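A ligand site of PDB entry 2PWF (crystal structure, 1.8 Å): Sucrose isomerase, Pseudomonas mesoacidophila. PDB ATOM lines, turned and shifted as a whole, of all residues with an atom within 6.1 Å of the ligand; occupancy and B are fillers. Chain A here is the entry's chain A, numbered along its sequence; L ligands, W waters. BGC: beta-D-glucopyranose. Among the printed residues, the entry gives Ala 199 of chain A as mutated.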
ATOM      1  N   TRP A  49      13.047   3.084  14.081  1.00  0.00           N
ATOM      2  CA  TRP A  49      12.790   2.397  12.801  1.00  0.00           C
ATOM      3  C   TRP A  49      11.319   1.950  12.940  1.00  0.00           C
ATOM      4  O   TRP A  49      10.919   1.318  13.938  1.00  0.00           O
ATOM      5  CB  TRP A  49      13.713   1.195  12.625  1.00  0.00           C
ATOM      6  CG  TRP A  49      13.169   0.141  11.630  1.00  0.00           C
ATOM      7  CD1 TRP A  49      12.414   0.365  10.512  1.00  0.00           C
ATOM      8  CD2 TRP A  49      13.290  -1.286  11.775  1.00  0.00           C
ATOM      9  NE1 TRP A  49      12.023  -0.848   9.967  1.00  0.00           N
ATOM     10  CE2 TRP A  49      12.538  -1.867  10.718  1.00  0.00           C
ATOM     11  CE3 TRP A  49      13.952  -2.128  12.693  1.00  0.00           C
ATOM     12  CZ2 TRP A  49      12.422  -3.253  10.555  1.00  0.00           C
ATOM     13  CZ3 TRP A  49      13.825  -3.497  12.542  1.00  0.00           C
ATOM     14  CH2 TRP A  49      13.063  -4.060  11.466  1.00  0.00           C
ATOM     15  N   ASN A  51       8.029  -0.034  11.174  1.00  0.00           N
ATOM     16  CA  ASN A  51       7.686  -1.040  10.202  1.00  0.00           C
ATOM     17  C   ASN A  51       6.897  -0.343   9.085  1.00  0.00           C
ATOM     18  O   ASN A  51       6.512   0.816   9.288  1.00  0.00           O
ATOM     19  CB  ASN A  51       6.973  -2.149  10.948  1.00  0.00           C
ATOM     20  CG  ASN A  51       7.982  -2.941  11.822  1.00  0.00           C
ATOM     21  OD1 ASN A  51       8.168  -2.673  13.008  1.00  0.00           O
ATOM     22  ND2 ASN A  51       8.693  -3.846  11.182  1.00  0.00           N
ATOM     23  N   ASP A  60       0.048  -9.016   4.806  1.00  0.00           N
ATOM     24  CA  ASP A  60       1.290  -9.278   5.593  1.00  0.00           C
ATOM     25  C   ASP A  60       1.652  -8.017   6.421  1.00  0.00           C
ATOM     26  O   ASP A  60       2.837  -7.620   6.515  1.00  0.00           O
ATOM     27  CB  ASP A  60       2.479  -9.664   4.670  1.00  0.00           C
ATOM     28  CG  ASP A  60       3.732 -10.123   5.439  1.00  0.00           C
ATOM     29  OD1 ASP A  60       3.642 -10.472   6.651  1.00  0.00           O
ATOM     30  OD2 ASP A  60       4.825 -10.107   4.842  1.00  0.00           O
ATOM     31  N   TYR A  63       3.767  -5.211   4.747  1.00  0.00           N
ATOM     32  CA  TYR A  63       4.771  -5.679   3.823  1.00  0.00           C
ATOM     33  C   TYR A  63       4.209  -6.029   2.445  1.00  0.00           C
ATOM     34  O   TYR A  63       4.937  -6.558   1.600  1.00  0.00           O
ATOM     35  CB  TYR A  63       5.553  -6.849   4.432  1.00  0.00           C
ATOM     36  CG  TYR A  63       6.485  -6.369   5.525  1.00  0.00           C
ATOM     37  CD1 TYR A  63       7.734  -5.807   5.205  1.00  0.00           C
ATOM     38  CD2 TYR A  63       6.115  -6.389   6.859  1.00  0.00           C
ATOM     39  CE1 TYR A  63       8.567  -5.288   6.179  1.00  0.00           C
ATOM     40  CE2 TYR A  63       6.970  -5.877   7.856  1.00  0.00           C
ATOM     41  CZ  TYR A  63       8.176  -5.324   7.497  1.00  0.00           C
ATOM     42  OH  TYR A  63       9.004  -4.796   8.462  1.00  0.00           O
ATOM     43  N   ASP A  64       2.901  -5.801   2.252  1.00  0.00           N
ATOM     44  CA  ASP A  64       2.281  -5.953   0.927  1.00  0.00           C
ATOM     45  C   ASP A  64       1.778  -4.546   0.558  1.00  0.00           C
ATOM     46  O   ASP A  64       0.649  -4.160   0.877  1.00  0.00           O
ATOM     47  CB  ASP A  64       1.136  -6.990   0.909  1.00  0.00           C
ATOM     48  CG  ASP A  64       0.087  -6.795   2.005  1.00  0.00           C
ATOM     49  OD1 ASP A  64       0.401  -6.417   3.185  1.00  0.00           O
ATOM     50  OD2 ASP A  64      -1.086  -7.093   1.651  1.00  0.00           O
ATOM     51  N   ASP A  98      10.876   1.552   6.702  1.00  0.00           N
ATOM     52  CA  ASP A  98      11.072   0.194   6.164  1.00  0.00           C
ATOM     53  C   ASP A  98      10.871   0.277   4.641  1.00  0.00           C
ATOM     54  O   ASP A  98       9.883   0.864   4.159  1.00  0.00           O
ATOM     55  CB  ASP A  98      10.023  -0.715   6.801  1.00  0.00           C
ATOM     56  CG  ASP A  98      10.526  -2.117   7.027  1.00  0.00           C
ATOM     57  OD1 ASP A  98      11.075  -2.699   6.069  1.00  0.00           O
ATOM     58  OD2 ASP A  98      10.384  -2.645   8.166  1.00  0.00           O
ATOM     59  N   VAL A 100      10.346  -1.867   1.202  1.00  0.00           N
ATOM     60  CA  VAL A 100       9.934  -3.215   0.771  1.00  0.00           C
ATOM     61  C   VAL A 100       9.877  -3.265  -0.759  1.00  0.00           C
ATOM     62  O   VAL A 100       8.817  -3.035  -1.380  1.00  0.00           O
ATOM     63  CB  VAL A 100       8.544  -3.542   1.363  1.00  0.00           C
ATOM     64  CG1 VAL A 100       8.219  -5.058   1.145  1.00  0.00           C
ATOM     65  CG2 VAL A 100       8.536  -3.200   2.884  1.00  0.00           C
ATOM     66  N   HIS A 103       9.140  -7.030  -3.438  1.00  0.00           N
ATOM     67  CA  HIS A 103       7.794  -7.351  -3.931  1.00  0.00           C
ATOM     68  C   HIS A 103       6.830  -6.250  -3.566  1.00  0.00           C
ATOM     69  O   HIS A 103       7.126  -5.404  -2.725  1.00  0.00           O
ATOM     70  CB  HIS A 103       7.273  -8.641  -3.264  1.00  0.00           C
ATOM     71  CG  HIS A 103       7.488  -8.674  -1.773  1.00  0.00           C
ATOM     72  ND1 HIS A 103       8.644  -9.167  -1.206  1.00  0.00           N
ATOM     73  CD2 HIS A 103       6.731  -8.234  -0.735  1.00  0.00           C
ATOM     74  CE1 HIS A 103       8.593  -9.046   0.103  1.00  0.00           C
ATOM     75  NE2 HIS A 103       7.432  -8.479   0.425  1.00  0.00           N
ATOM     76  N   PHE A 144       5.412 -18.457   2.788  1.00  0.00           N
ATOM     77  CA  PHE A 144       4.073 -18.422   3.346  1.00  0.00           C
ATOM     78  C   PHE A 144       3.139 -19.532   2.856  1.00  0.00           C
ATOM     79  O   PHE A 144       1.919 -19.422   2.968  1.00  0.00           O
ATOM     80  CB  PHE A 144       3.428 -17.037   3.105  1.00  0.00           C
ATOM     81  CG  PHE A 144       4.143 -15.933   3.823  1.00  0.00           C
ATOM     82  CD1 PHE A 144       5.144 -16.219   4.769  1.00  0.00           C
ATOM     83  CD2 PHE A 144       3.804 -14.594   3.583  1.00  0.00           C
ATOM     84  CE1 PHE A 144       5.795 -15.193   5.456  1.00  0.00           C
ATOM     85  CE2 PHE A 144       4.446 -13.559   4.274  1.00  0.00           C
ATOM     86  CZ  PHE A 144       5.448 -13.859   5.206  1.00  0.00           C
ATOM     87  N   PHE A 163       7.151 -14.668  -1.154  1.00  0.00           N
ATOM     88  CA  PHE A 163       6.371 -14.602   0.072  1.00  0.00           C
ATOM     89  C   PHE A 163       4.918 -14.908  -0.212  1.00  0.00           C
ATOM     90  O   PHE A 163       4.639 -15.942  -0.844  1.00  0.00           O
ATOM     91  CB  PHE A 163       6.599 -13.267   0.812  1.00  0.00           C
ATOM     92  CG  PHE A 163       8.002 -13.121   1.327  1.00  0.00           C
ATOM     93  CD1 PHE A 163       9.027 -12.706   0.478  1.00  0.00           C
ATOM     94  CD2 PHE A 163       8.327 -13.512   2.632  1.00  0.00           C
ATOM     95  CE1 PHE A 163      10.380 -12.709   0.906  1.00  0.00           C
ATOM     96  CE2 PHE A 163       9.675 -13.515   3.074  1.00  0.00           C
ATOM     97  CZ  PHE A 163      10.684 -13.118   2.227  1.00  0.00           C
ATOM     98  N   GLN A 167       1.825 -10.972  -2.740  1.00  0.00           N
ATOM     99  CA  GLN A 167       3.072 -10.199  -2.706  1.00  0.00           C
ATOM    100  C   GLN A 167       3.946 -10.623  -3.897  1.00  0.00           C
ATOM    101  O   GLN A 167       5.004 -11.272  -3.737  1.00  0.00           O
ATOM    102  CB  GLN A 167       3.829 -10.462  -1.383  1.00  0.00           C
ATOM    103  CG  GLN A 167       3.187  -9.759  -0.151  1.00  0.00           C
ATOM    104  CD  GLN A 167       3.720 -10.315   1.187  1.00  0.00           C
ATOM    105  OE1 GLN A 167       3.414 -11.464   1.579  1.00  0.00           O
ATOM    106  NE2 GLN A 167       4.530  -9.512   1.858  1.00  0.00           N
ATOM    107  N   ARG A 197      15.540   0.817   6.077  1.00  0.00           N
ATOM    108  CA  ARG A 197      15.810  -0.578   6.405  1.00  0.00           C
ATOM    109  C   ARG A 197      15.235  -1.354   5.210  1.00  0.00           C
ATOM    110  O   ARG A 197      14.029  -1.249   4.897  1.00  0.00           O
ATOM    111  CB  ARG A 197      15.068  -0.989   7.675  1.00  0.00           C
ATOM    112  CG  ARG A 197      15.174  -2.456   7.980  1.00  0.00           C
ATOM    113  CD  ARG A 197      13.980  -3.254   7.491  1.00  0.00           C
ATOM    114  NE  ARG A 197      13.965  -4.561   8.143  1.00  0.00           N
ATOM    115  CZ  ARG A 197      13.086  -5.521   7.877  1.00  0.00           C
ATOM    116  NH1 ARG A 197      12.126  -5.298   6.983  1.00  0.00           N
ATOM    117  NH2 ARG A 197      13.144  -6.705   8.503  1.00  0.00           N
ATOM    118  N   PHE A 198      16.085  -2.122   4.554  1.00  0.00           N
ATOM    119  CA  PHE A 198      15.659  -2.860   3.370  1.00  0.00           C
ATOM    120  C   PHE A 198      15.237  -4.284   3.621  1.00  0.00           C
ATOM    121  O   PHE A 198      16.090  -5.148   3.864  1.00  0.00           O
ATOM    122  CB  PHE A 198      16.772  -2.856   2.328  1.00  0.00           C
ATOM    123  CG  PHE A 198      17.043  -1.482   1.771  1.00  0.00           C
ATOM    124  CD1 PHE A 198      17.708  -0.525   2.554  1.00  0.00           C
ATOM    125  CD2 PHE A 198      16.535  -1.121   0.526  1.00  0.00           C
ATOM    126  CE1 PHE A 198      17.859   0.794   2.104  1.00  0.00           C
ATOM    127  CE2 PHE A 198      16.686   0.207   0.053  1.00  0.00           C
ATOM    128  CZ  PHE A 198      17.329   1.156   0.827  1.00  0.00           C
ATOM    129  N   ALA A 199      13.922  -4.508   3.554  1.00  0.00           N
ATOM    130  CA  ALA A 199      13.325  -5.819   3.703  1.00  0.00           C
ATOM    131  C   ALA A 199      13.875  -6.832   2.686  1.00  0.00           C
ATOM    132  O   ALA A 199      13.927  -6.554   1.468  1.00  0.00           O
ATOM    133  CB  ALA A 199      11.819  -5.722   3.512  1.00  0.00           C
ATOM    134  N   THR A 200      14.255  -8.008   3.220  1.00  0.00           N
ATOM    135  CA  THR A 200      14.770  -9.119   2.432  1.00  0.00           C
ATOM    136  C   THR A 200      15.582  -8.611   1.218  1.00  0.00           C
ATOM    137  O   THR A 200      15.338  -8.925   0.040  1.00  0.00           O
ATOM    138  CB  THR A 200      13.582 -10.137   2.044  1.00  0.00           C
ATOM    139  OG1 THR A 200      14.153 -11.247   1.344  1.00  0.00           O
ATOM    140  CG2 THR A 200      12.474  -9.508   1.118  1.00  0.00           C
ATOM    141  N   GLU A 253      18.239  -6.027   5.623  1.00  0.00           N
ATOM    142  CA  GLU A 253      17.776  -7.231   6.311  1.00  0.00           C
ATOM    143  C   GLU A 253      18.270  -8.356   5.395  1.00  0.00           C
ATOM    144  O   GLU A 253      17.645  -8.683   4.347  1.00  0.00           O
ATOM    145  CB  GLU A 253      16.253  -7.338   6.439  1.00  0.00           C
ATOM    146  CG  GLU A 253      15.835  -8.642   7.174  1.00  0.00           C
ATOM    147  CD  GLU A 253      14.444  -9.114   6.876  1.00  0.00           C
ATOM    148  OE1 GLU A 253      13.971  -8.872   5.749  1.00  0.00           O
ATOM    149  OE2 GLU A 253      13.838  -9.771   7.760  1.00  0.00           O
ATOM    150  N   ASN A 324      12.662  -8.524  17.424  1.00  0.00           N
ATOM    151  CA  ASN A 324      12.044  -7.717  16.363  1.00  0.00           C
ATOM    152  C   ASN A 324      10.639  -8.248  16.120  1.00  0.00           C
ATOM    153  O   ASN A 324      10.163  -9.076  16.864  1.00  0.00           O
ATOM    154  CB  ASN A 324      12.884  -7.680  15.046  1.00  0.00           C
ATOM    155  CG  ASN A 324      12.942  -9.024  14.269  1.00  0.00           C
ATOM    156  OD1 ASN A 324      12.150  -9.965  14.428  1.00  0.00           O
ATOM    157  ND2 ASN A 324      13.921  -9.072  13.344  1.00  0.00           N
ATOM    158  N   HIS A 325       9.986  -7.797  15.061  1.00  0.00           N
ATOM    159  CA  HIS A 325       8.579  -8.177  14.840  1.00  0.00           C
ATOM    160  C   HIS A 325       8.383  -9.540  14.172  1.00  0.00           C
ATOM    161  O   HIS A 325       7.249  -9.952  13.961  1.00  0.00           O
ATOM    162  CB  HIS A 325       7.919  -7.150  13.952  1.00  0.00           C
ATOM    163  CG  HIS A 325       8.556  -7.094  12.605  1.00  0.00           C
ATOM    164  ND1 HIS A 325       9.873  -6.712  12.423  1.00  0.00           N
ATOM    165  CD2 HIS A 325       8.099  -7.474  11.394  1.00  0.00           C
ATOM    166  CE1 HIS A 325      10.199  -6.861  11.149  1.00  0.00           C
ATOM    167  NE2 HIS A 325       9.135  -7.334  10.504  1.00  0.00           N
ATOM    168  N   ASP A 326       9.487 -10.219  13.867  1.00  0.00           N
ATOM    169  CA  ASP A 326       9.403 -11.542  13.218  1.00  0.00           C
ATOM    170  C   ASP A 326       9.874 -12.667  14.133  1.00  0.00           C
ATOM    171  O   ASP A 326      10.035 -13.799  13.666  1.00  0.00           O
ATOM    172  CB  ASP A 326      10.307 -11.574  11.947  1.00  0.00           C
ATOM    173  CG  ASP A 326       9.794 -10.669  10.820  1.00  0.00           C
ATOM    174  OD1 ASP A 326       8.585 -10.430  10.754  1.00  0.00           O
ATOM    175  OD2 ASP A 326      10.609 -10.230   9.991  1.00  0.00           O
ATOM    176  N   ARG A 413       5.907 -15.153  15.080  1.00  0.00           N
ATOM    177  CA  ARG A 413       6.128 -13.712  14.996  1.00  0.00           C
ATOM    178  C   ARG A 413       5.066 -12.990  15.807  1.00  0.00           C
ATOM    179  O   ARG A 413       5.287 -11.857  16.281  1.00  0.00           O
ATOM    180  CB  ARG A 413       6.009 -13.260  13.532  1.00  0.00           C
ATOM    181  CG  ARG A 413       6.899 -14.065  12.597  1.00  0.00           C
ATOM    182  CD  ARG A 413       7.139 -13.453  11.222  1.00  0.00           C
ATOM    183  NE  ARG A 413       5.937 -13.393  10.397  1.00  0.00           N
ATOM    184  CZ  ARG A 413       5.872 -12.773   9.226  1.00  0.00           C
ATOM    185  NH1 ARG A 413       6.944 -12.144   8.749  1.00  0.00           N
ATOM    186  NH2 ARG A 413       4.748 -12.805   8.513  1.00  0.00           N
ATOM    187  N   ARG A 417       4.120  -9.237  18.432  1.00  0.00           N
ATOM    188  CA  ARG A 417       3.087  -8.290  17.934  1.00  0.00           C
ATOM    189  C   ARG A 417       1.894  -7.989  18.840  1.00  0.00           C
ATOM    190  O   ARG A 417       0.994  -7.241  18.467  1.00  0.00           O
ATOM    191  CB  ARG A 417       2.579  -8.837  16.598  1.00  0.00           C
ATOM    192  CG  ARG A 417       3.756  -9.041  15.626  1.00  0.00           C
ATOM    193  CD  ARG A 417       3.301  -9.685  14.347  1.00  0.00           C
ATOM    194  NE  ARG A 417       4.434  -9.877  13.441  1.00  0.00           N
ATOM    195  CZ  ARG A 417       4.321  -9.976  12.117  1.00  0.00           C
ATOM    196  NH1 ARG A 417       3.121  -9.920  11.519  1.00  0.00           N
ATOM    197  NH2 ARG A 417       5.417 -10.079  11.371  1.00  0.00           N
HETATM  198  C2  BGC L   1       9.783  -8.562   7.162  1.00  0.00           C
HETATM  199  C3  BGC L   1       8.694  -9.611   7.399  1.00  0.00           C
HETATM  200  C4  BGC L   1       7.888  -9.804   6.103  1.00  0.00           C
HETATM  201  C5  BGC L   1       8.832 -10.189   4.953  1.00  0.00           C
HETATM  202  C6  BGC L   1       8.114 -10.217   3.622  1.00  0.00           C
HETATM  203  C1  BGC L   1      10.674  -9.037   6.008  1.00  0.00           C
HETATM  204  O1  BGC L   1      11.641  -8.069   5.749  1.00  0.00           O
HETATM  205  O2  BGC L   1      10.580  -8.378   8.327  1.00  0.00           O
HETATM  206  O3  BGC L   1       7.826  -9.198   8.449  1.00  0.00           O
HETATM  207  O4  BGC L   1       6.910 -10.821   6.268  1.00  0.00           O
HETATM  208  O5  BGC L   1       9.886  -9.221   4.817  1.00  0.00           O
HETATM  209  O6  BGC L   1       7.702  -8.911   3.264  1.00  0.00           O
HETATM  210  O   HOH W   1       5.134  -9.220   8.594  1.00  0.00           O
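Water W1 lies within hydrogen-bond range of an oxygen (O3) of the ligand, the side-chain carboxylate (OD1) of Asp 60, the guanidinium group (NH2) of Arg 417 and the guanidinium group (NH1) of Arg 413.
Residues that only touch the ligand: Tyr 63, Ala 199, Phe 163, Gln 167, Phe 144, Thr 200 and Arg 417.
Hydrophobic or aromatic side chains that line the ligand: Tyr 63, His 103, Phe 144, Phe 163, Ala 199 and His 325.
14 residues have an atom within 4 Å of the ligand: Asp 60, Tyr 63, His 103, Phe 144, Phe 163, Gln 167, Arg 197, Ala 199, Thr 200, Glu 253, His 325, Asp 326, Arg 413 and Arg 417.
The nearest printed residue that does not touch the ligand is Val 100 (4.4 Å).
The side-chain carboxylate (OE1) of Glu 253 lies within hydrogen-bond range of an oxygen (O1) of the ligand, at 2.5 Å.
The side-chain carboxylate (OD2) of Asp 326 sits at hydrogen-bond distance from an oxygen (O2) of the ligand.
The side-chain carboxylate (OD2) of Asp 60 lies within hydrogen-bond range of an oxygen (O4) of the ligand, at 2.6 Å.
O4 of the ligand is in hydrogen-bond range of NH1 of Arg 413 (2.8 Å).
A ring nitrogen (NE2) of His 325 is in hydrogen-bond range of an oxygen (O2) of the ligand.
NE2 of His 103 is in hydrogen-bond range of O6 of the ligand.
The guanidinium group (NH2) of Arg 197 sits at hydrogen-bond distance from an oxygen (O2) of the ligand, 3.1 Å away.
NE2 of His 325 lies close to OD1 of Asp 326.
The backbone NH (N) of Asp 326 is in hydrogen-bond range of the side-chain amide oxygen (OD1) of Asn 324 (2.7 Å).
OD1 of Asp 60 is in salt-bridge range of NH2 of Arg 413.
NE2 of His 325 is in hydrogen-bond range of OH of Tyr 63 (3.3 Å).
The backbone carbonyl oxygen (O) of His 325 is in hydrogen-bond range of the guanidinium group (NE) of Arg 417, 2.9 Å away.
ND1 of His 325 is in hydrogen-bond range of ND2 of Asn 51 (3.3 Å).
A ring nitrogen (NE2) of His 103 is in hydrogen-bond range of the side-chain amide nitrogen of Gln 167, 3.4 Å away.
The side-chain carboxylate of Asp 98 is in hydrogen-bond range of the side-chain hydroxyl of Tyr 63.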
